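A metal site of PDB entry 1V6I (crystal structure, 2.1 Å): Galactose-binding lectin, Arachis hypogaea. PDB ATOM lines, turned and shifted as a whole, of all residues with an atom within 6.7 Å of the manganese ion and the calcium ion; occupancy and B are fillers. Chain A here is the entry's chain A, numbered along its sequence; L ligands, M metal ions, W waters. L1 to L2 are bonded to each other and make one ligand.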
ATOM      1  N   ASP A  83       8.870   3.679 -20.122  1.00  0.00           N
ATOM      2  CA  ASP A  83       9.706   3.040 -21.151  1.00  0.00           C
ATOM      3  C   ASP A  83       9.900   1.547 -20.907  1.00  0.00           C
ATOM      4  O   ASP A  83      10.173   0.786 -21.839  1.00  0.00           O
ATOM      5  CB  ASP A  83      11.072   3.714 -21.216  1.00  0.00           C
ATOM      6  CG  ASP A  83      11.121   4.851 -22.220  1.00  0.00           C
ATOM      7  OD1 ASP A  83      11.248   4.576 -23.422  1.00  0.00           O
ATOM      8  OD2 ASP A  83      11.032   6.022 -21.795  1.00  0.00           O
ATOM      9  N   GLY A 103      14.501   7.482 -20.630  1.00  0.00           N
ATOM     10  CA  GLY A 103      13.870   6.997 -21.836  1.00  0.00           C
ATOM     11  C   GLY A 103      14.259   5.590 -22.259  1.00  0.00           C
ATOM     12  O   GLY A 103      14.286   4.669 -21.435  1.00  0.00           O
ATOM     13  N   GLY A 104      14.583   5.436 -23.542  1.00  0.00           N
ATOM     14  CA  GLY A 104      14.965   4.147 -24.080  1.00  0.00           C
ATOM     15  C   GLY A 104      16.261   3.530 -23.578  1.00  0.00           C
ATOM     16  O   GLY A 104      16.542   2.370 -23.879  1.00  0.00           O
ATOM     17  N   THR A 105      17.053   4.288 -22.830  1.00  0.00           N
ATOM     18  CA  THR A 105      18.315   3.764 -22.317  1.00  0.00           C
ATOM     19  C   THR A 105      18.042   2.855 -21.114  1.00  0.00           C
ATOM     20  O   THR A 105      18.922   2.155 -20.638  1.00  0.00           O
ATOM     21  CB  THR A 105      19.275   4.899 -21.858  1.00  0.00           C
ATOM     22  OG1 THR A 105      18.758   5.508 -20.672  1.00  0.00           O
ATOM     23  CG2 THR A 105      19.395   5.953 -22.949  1.00  0.00           C
ATOM     24  N   LEU A 106      16.795   2.890 -20.637  1.00  0.00           N
ATOM     25  CA  LEU A 106      16.342   2.100 -19.510  1.00  0.00           C
ATOM     26  C   LEU A 106      17.152   2.287 -18.230  1.00  0.00           C
ATOM     27  O   LEU A 106      17.125   1.439 -17.327  1.00  0.00           O
ATOM     28  CB  LEU A 106      16.295   0.605 -19.911  1.00  0.00           C
ATOM     29  CG  LEU A 106      15.296   0.318 -21.048  1.00  0.00           C
ATOM     30  CD1 LEU A 106      15.313  -1.151 -21.420  1.00  0.00           C
ATOM     31  CD2 LEU A 106      13.902   0.722 -20.616  1.00  0.00           C
ATOM     32  N   GLU A 121      15.303  -7.273 -20.660  1.00  0.00           N
ATOM     33  CA  GLU A 121      14.419  -6.114 -20.684  1.00  0.00           C
ATOM     34  C   GLU A 121      12.971  -6.420 -21.040  1.00  0.00           C
ATOM     35  O   GLU A 121      12.666  -7.354 -21.800  1.00  0.00           O
ATOM     36  CB  GLU A 121      14.966  -5.059 -21.653  1.00  0.00           C
ATOM     37  CG  GLU A 121      15.104  -5.540 -23.079  1.00  0.00           C
ATOM     38  CD  GLU A 121      15.319  -4.406 -24.063  1.00  0.00           C
ATOM     39  OE1 GLU A 121      16.304  -3.665 -23.928  1.00  0.00           O
ATOM     40  OE2 GLU A 121      14.482  -4.265 -24.972  1.00  0.00           O
ATOM     41  N   ASP A 123      10.554  -4.187 -22.485  1.00  0.00           N
ATOM     42  CA  ASP A 123      10.464  -2.936 -23.205  1.00  0.00           C
ATOM     43  C   ASP A 123       9.081  -2.558 -23.742  1.00  0.00           C
ATOM     44  O   ASP A 123       8.532  -3.272 -24.580  1.00  0.00           O
ATOM     45  CB  ASP A 123      11.455  -3.019 -24.362  1.00  0.00           C
ATOM     46  CG  ASP A 123      11.919  -1.683 -24.789  1.00  0.00           C
ATOM     47  OD1 ASP A 123      11.144  -0.718 -24.641  1.00  0.00           O
ATOM     48  OD2 ASP A 123      13.065  -1.601 -25.281  1.00  0.00           O
ATOM     49  N   THR A 124       8.559  -1.417 -23.301  1.00  0.00           N
ATOM     50  CA  THR A 124       7.225  -0.990 -23.728  1.00  0.00           C
ATOM     51  C   THR A 124       7.148   0.138 -24.757  1.00  0.00           C
ATOM     52  O   THR A 124       6.070   0.619 -25.060  1.00  0.00           O
ATOM     53  CB  THR A 124       6.377  -0.563 -22.512  1.00  0.00           C
ATOM     54  OG1 THR A 124       6.903   0.655 -21.980  1.00  0.00           O
ATOM     55  CG2 THR A 124       6.409  -1.644 -21.435  1.00  0.00           C
ATOM     56  N   TYR A 125       8.281   0.573 -25.280  1.00  0.00           N
ATOM     57  CA  TYR A 125       8.258   1.638 -26.296  1.00  0.00           C
ATOM     58  C   TYR A 125       9.288   1.337 -27.372  1.00  0.00           C
ATOM     59  O   TYR A 125      10.391   0.911 -27.063  1.00  0.00           O
ATOM     60  CB  TYR A 125       8.540   3.006 -25.673  1.00  0.00           C
ATOM     61  CG  TYR A 125       8.587   4.101 -26.710  1.00  0.00           C
ATOM     62  CD1 TYR A 125       9.764   4.364 -27.419  1.00  0.00           C
ATOM     63  CD2 TYR A 125       7.441   4.836 -27.035  1.00  0.00           C
ATOM     64  CE1 TYR A 125       9.798   5.318 -28.426  1.00  0.00           C
ATOM     65  CE2 TYR A 125       7.467   5.796 -28.042  1.00  0.00           C
ATOM     66  CZ  TYR A 125       8.646   6.030 -28.733  1.00  0.00           C
ATOM     67  OH  TYR A 125       8.682   6.970 -29.730  1.00  0.00           O
ATOM     68  N   SER A 126       8.952   1.570 -28.629  1.00  0.00           N
ATOM     69  CA  SER A 126       9.889   1.256 -29.696  1.00  0.00           C
ATOM     70  C   SER A 126      10.835   2.378 -30.097  1.00  0.00           C
ATOM     71  O   SER A 126      10.460   3.276 -30.844  1.00  0.00           O
ATOM     72  CB  SER A 126       9.106   0.778 -30.920  1.00  0.00           C
ATOM     73  OG  SER A 126       9.982   0.481 -31.993  1.00  0.00           O
ATOM     74  N   ASN A 127      12.072   2.318 -29.588  1.00  0.00           N
ATOM     75  CA  ASN A 127      13.083   3.327 -29.929  1.00  0.00           C
ATOM     76  C   ASN A 127      13.820   2.843 -31.161  1.00  0.00           C
ATOM     77  O   ASN A 127      14.625   1.912 -31.092  1.00  0.00           O
ATOM     78  CB  ASN A 127      14.110   3.512 -28.804  1.00  0.00           C
ATOM     79  CG  ASN A 127      13.508   4.058 -27.531  1.00  0.00           C
ATOM     80  OD1 ASN A 127      12.903   3.323 -26.762  1.00  0.00           O
ATOM     81  ND2 ASN A 127      13.654   5.356 -27.312  1.00  0.00           N
ATOM     82  N   TYR A 130      17.633   2.493 -31.288  1.00  0.00           N
ATOM     83  CA  TYR A 130      18.281   1.322 -30.667  1.00  0.00           C
ATOM     84  C   TYR A 130      17.801   0.047 -31.359  1.00  0.00           C
ATOM     85  O   TYR A 130      17.881  -1.040 -30.801  1.00  0.00           O
ATOM     86  CB  TYR A 130      17.958   1.252 -29.176  1.00  0.00           C
ATOM     87  CG  TYR A 130      18.356   2.486 -28.406  1.00  0.00           C
ATOM     88  CD1 TYR A 130      19.632   3.020 -28.511  1.00  0.00           C
ATOM     89  CD2 TYR A 130      17.434   3.151 -27.588  1.00  0.00           C
ATOM     90  CE1 TYR A 130      19.991   4.185 -27.841  1.00  0.00           C
ATOM     91  CE2 TYR A 130      17.791   4.315 -26.897  1.00  0.00           C
ATOM     92  CZ  TYR A 130      19.067   4.829 -27.034  1.00  0.00           C
ATOM     93  OH  TYR A 130      19.423   5.987 -26.385  1.00  0.00           O
ATOM     94  N   ASN A 131      17.298   0.216 -32.580  1.00  0.00           N
ATOM     95  CA  ASN A 131      16.808  -0.890 -33.393  1.00  0.00           C
ATOM     96  C   ASN A 131      15.766  -1.782 -32.717  1.00  0.00           C
ATOM     97  O   ASN A 131      15.771  -2.994 -32.882  1.00  0.00           O
ATOM     98  CB  ASN A 131      17.984  -1.748 -33.870  1.00  0.00           C
ATOM     99  CG  ASN A 131      19.012  -0.943 -34.644  1.00  0.00           C
ATOM    100  OD1 ASN A 131      18.654  -0.180 -35.538  1.00  0.00           O
ATOM    101  ND2 ASN A 131      20.282  -1.119 -34.320  1.00  0.00           N
ATOM    102  N   ASP A 132      14.860  -1.155 -31.960  1.00  0.00           N
ATOM    103  CA  ASP A 132      13.810  -1.896 -31.275  1.00  0.00           C
ATOM    104  C   ASP A 132      12.810  -2.522 -32.231  1.00  0.00           C
ATOM    105  O   ASP A 132      12.604  -2.024 -33.335  1.00  0.00           O
ATOM    106  CB  ASP A 132      12.994  -0.975 -30.367  1.00  0.00           C
ATOM    107  CG  ASP A 132      13.563  -0.848 -28.989  1.00  0.00           C
ATOM    108  OD1 ASP A 132      14.195  -1.808 -28.508  1.00  0.00           O
ATOM    109  OD2 ASP A 132      13.355   0.205 -28.374  1.00  0.00           O
ATOM    110  N   PRO A 133      12.177  -3.625 -31.811  1.00  0.00           N
ATOM    111  CA  PRO A 133      11.188  -4.244 -32.695  1.00  0.00           C
ATOM    112  C   PRO A 133      10.031  -3.250 -32.672  1.00  0.00           C
ATOM    113  O   PRO A 133      10.019  -2.331 -31.850  1.00  0.00           O
ATOM    114  CB  PRO A 133      10.844  -5.546 -31.970  1.00  0.00           C
ATOM    115  CG  PRO A 133      12.088  -5.852 -31.203  1.00  0.00           C
ATOM    116  CD  PRO A 133      12.487  -4.501 -30.667  1.00  0.00           C
ATOM    117  N   HIS A 137       8.238  -5.795 -26.204  1.00  0.00           N
ATOM    118  CA  HIS A 137       9.047  -6.992 -26.322  1.00  0.00           C
ATOM    119  C   HIS A 137       9.935  -7.293 -25.123  1.00  0.00           C
ATOM    120  O   HIS A 137      10.165  -6.457 -24.257  1.00  0.00           O
ATOM    121  CB  HIS A 137       9.955  -6.865 -27.547  1.00  0.00           C
ATOM    122  CG  HIS A 137      10.765  -5.613 -27.553  1.00  0.00           C
ATOM    123  ND1 HIS A 137      10.221  -4.376 -27.845  1.00  0.00           N
ATOM    124  CD2 HIS A 137      12.061  -5.394 -27.242  1.00  0.00           C
ATOM    125  CE1 HIS A 137      11.162  -3.449 -27.704  1.00  0.00           C
ATOM    126  NE2 HIS A 137      12.282  -4.039 -27.343  1.00  0.00           N
ATOM    127  N   VAL A 138      10.428  -8.530 -25.100  1.00  0.00           N
ATOM    128  CA  VAL A 138      11.352  -8.975 -24.068  1.00  0.00           C
ATOM    129  C   VAL A 138      12.649  -9.169 -24.852  1.00  0.00           C
ATOM    130  O   VAL A 138      12.630  -9.686 -25.976  1.00  0.00           O
ATOM    131  CB  VAL A 138      10.916 -10.320 -23.457  1.00  0.00           C
ATOM    132  CG1 VAL A 138      11.942 -10.774 -22.422  1.00  0.00           C
ATOM    133  CG2 VAL A 138       9.545 -10.179 -22.806  1.00  0.00           C
ATOM    134  N   GLY A 139      13.763  -8.743 -24.297  1.00  0.00           N
ATOM    135  CA  GLY A 139      15.008  -8.900 -25.014  1.00  0.00           C
ATOM    136  C   GLY A 139      16.174  -9.198 -24.105  1.00  0.00           C
ATOM    137  O   GLY A 139      16.132  -8.905 -22.911  1.00  0.00           O
ATOM    138  N   ASP A 141      19.896  -8.313 -23.399  1.00  0.00           N
ATOM    139  CA  ASP A 141      20.858  -7.259 -23.662  1.00  0.00           C
ATOM    140  C   ASP A 141      22.254  -7.583 -23.140  1.00  0.00           C
ATOM    141  O   ASP A 141      22.413  -8.020 -21.997  1.00  0.00           O
ATOM    142  CB  ASP A 141      20.393  -5.939 -23.030  1.00  0.00           C
ATOM    143  CG  ASP A 141      19.063  -5.449 -23.584  1.00  0.00           C
ATOM    144  OD1 ASP A 141      18.599  -5.936 -24.629  1.00  0.00           O
ATOM    145  OD2 ASP A 141      18.467  -4.539 -22.954  1.00  0.00           O
ATOM    146  N   VAL A 145      21.425  -1.628 -25.273  1.00  0.00           N
ATOM    147  CA  VAL A 145      19.973  -1.754 -25.264  1.00  0.00           C
ATOM    148  C   VAL A 145      19.520  -2.160 -26.666  1.00  0.00           C
ATOM    149  O   VAL A 145      18.327  -2.294 -26.949  1.00  0.00           O
ATOM    150  CB  VAL A 145      19.276  -0.444 -24.843  1.00  0.00           C
ATOM    151  CG1 VAL A 145      19.474  -0.209 -23.341  1.00  0.00           C
ATOM    152  CG2 VAL A 145      19.810   0.718 -25.645  1.00  0.00           C
ATOM    153  N   ASP A 146      20.496  -2.320 -27.547  1.00  0.00           N
ATOM    154  CA  ASP A 146      20.224  -2.793 -28.901  1.00  0.00           C
ATOM    155  C   ASP A 146      20.344  -4.287 -28.646  1.00  0.00           C
ATOM    156  O   ASP A 146      21.422  -4.868 -28.743  1.00  0.00           O
ATOM    157  CB  ASP A 146      21.318  -2.342 -29.871  1.00  0.00           C
ATOM    158  CG  ASP A 146      20.999  -2.713 -31.305  1.00  0.00           C
ATOM    159  OD1 ASP A 146      20.340  -3.753 -31.540  1.00  0.00           O
ATOM    160  OD2 ASP A 146      21.412  -1.975 -32.219  1.00  0.00           O
ATOM    161  N   SER A 147      19.216  -4.895 -28.285  1.00  0.00           N
ATOM    162  CA  SER A 147      19.158  -6.319 -27.946  1.00  0.00           C
ATOM    163  C   SER A 147      19.799  -7.294 -28.928  1.00  0.00           C
ATOM    164  O   SER A 147      19.694  -7.161 -30.144  1.00  0.00           O
ATOM    165  CB  SER A 147      17.699  -6.735 -27.724  1.00  0.00           C
ATOM    166  OG  SER A 147      17.100  -5.978 -26.680  1.00  0.00           O
ATOM    167  N   THR A 150      15.342 -10.575 -29.326  1.00  0.00           N
ATOM    168  CA  THR A 150      14.063 -10.146 -28.758  1.00  0.00           C
ATOM    169  C   THR A 150      12.958 -11.095 -29.162  1.00  0.00           C
ATOM    170  O   THR A 150      13.120 -11.879 -30.099  1.00  0.00           O
ATOM    171  CB  THR A 150      13.639  -8.734 -29.226  1.00  0.00           C
ATOM    172  OG1 THR A 150      13.319  -8.781 -30.630  1.00  0.00           O
ATOM    173  CG2 THR A 150      14.753  -7.718 -28.988  1.00  0.00           C
HETATM  174  C1  LIG L   1      10.051  14.784 -27.405  1.00  0.00           C
HETATM  175  C2  LIG L   1       9.184  14.129 -26.319  1.00  0.00           C
HETATM  176  C3  LIG L   1       9.933  12.970 -25.655  1.00  0.00           C
HETATM  177  C4  LIG L   1      10.438  11.999 -26.714  1.00  0.00           C
HETATM  178  C5  LIG L   1      11.301  12.766 -27.722  1.00  0.00           C
HETATM  179  C6  LIG L   1      11.865  11.896 -28.828  1.00  0.00           C
HETATM  180  O1  LIG L   1      11.157  15.381 -26.821  1.00  0.00           O
HETATM  181  O2  LIG L   1       8.857  15.102 -25.340  1.00  0.00           O
HETATM  182  O3  LIG L   1       9.062  12.285 -24.763  1.00  0.00           O
HETATM  183  O4  LIG L   1      11.211  10.962 -26.089  1.00  0.00           O
HETATM  184  O5  LIG L   1      10.527  13.804 -28.347  1.00  0.00           O
HETATM  185  O6  LIG L   1      10.845  11.138 -29.443  1.00  0.00           O
HETATM  186  C1  LG2 L   2      10.796   9.660 -26.301  1.00  0.00           C
HETATM  187  C2  LG2 L   2      11.806   8.705 -25.663  1.00  0.00           C
HETATM  188  C3  LG2 L   2      11.295   7.262 -25.703  1.00  0.00           C
HETATM  189  C4  LG2 L   2       9.889   7.188 -25.080  1.00  0.00           C
HETATM  190  C5  LG2 L   2       8.986   8.161 -25.835  1.00  0.00           C
HETATM  191  C6  LG2 L   2       7.558   8.165 -25.321  1.00  0.00           C
HETATM  192  O1  LG2 L   2      13.039   8.783 -26.357  1.00  0.00           O
HETATM  193  O2  LG2 L   2      12.185   6.425 -24.991  1.00  0.00           O
HETATM  194  O3  LG2 L   2       9.947   7.559 -23.708  1.00  0.00           O
HETATM  195  O4  LG2 L   2       9.500   9.493 -25.700  1.00  0.00           O
HETATM  196  O5  LG2 L   2       6.670   8.688 -26.294  1.00  0.00           O
HETATM  197 MN    MN M   1      14.175  -2.928 -26.652  1.00  0.00          MN
HETATM  198 CA    CA M   2      12.646   0.877 -26.046  1.00  0.00          CA
HETATM  199  O   HOH W   1      15.428  -4.411 -27.945  1.00  0.00           O
HETATM  200  O   HOH W   2      11.861   2.061 -23.898  1.00  0.00           O
HETATM  201  O   HOH W   3      15.137   0.748 -25.461  1.00  0.00           O
HETATM  202  O   HOH W   4      16.017  -1.798 -25.775  1.00  0.00           O
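Of the 23 residues printed, 4 come within 4 Å of the calcium ion.
The nearest printed residue that does not touch the calcium ion is Gly 104 (4.5 Å).
The manganese ion is bound by OD1 of Asp 132 (2.2 Å), OE2 of Glu 121 (2.2 Å), OD2 of Asp 123 (2.2 Å), NE2 of His 137 (2.3 Å), water W1 (2.3 Å) and water W4 (2.3 Å).
An oxygen (O2) of LG2 L2 sits at hydrogen-bond distance from the backbone NH (N) of Gly 104, 3.0 Å away.
An oxygen (O2) of LG2 L2 is in hydrogen-bond range of the side-chain amide nitrogen (ND2) of Asn 127, at 2.9 Å.
An oxygen (O2) of LG2 L2 is in hydrogen-bond range of the side-chain carboxylate (OD1) of Asp 83 (2.6 Å).
Along chain A the residues within 4 Å of the manganese ion span positions 121 to 137.
The nearest printed residue that does not touch the manganese ion is Val 145 (4.2 Å).
The calcium ion is bound by the backbone carbonyl oxygen (O) of Tyr 125 (2.5 Å).
The side-chain carboxylate (OD2) of Asp 132 binds the calcium ion, at 2.5 Å.
OD1 of Asn 127 is bound to the calcium ion, at 2.6 Å.
Water W3 is bound to the calcium ion (2.6 Å).
Water W2 is bound to the calcium ion, 2.6 Å away.
The side-chain carboxylate (OD1) of Asp 123 binds the calcium ion, at 2.6 Å.
The side-chain carboxylate (OD2) of Asp 123 is bound to the calcium ion, at 2.6 Å.
Water W4 bridges the backbone carbonyl oxygen (O) of Val 145 and the side-chain carboxylate (OE1) of Glu 121.
N of Glu 121 lies within hydrogen-bond range of O of Gly 139 (2.9 Å).
OD2 of Asp 141 lies close to OE1 of Glu 121.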
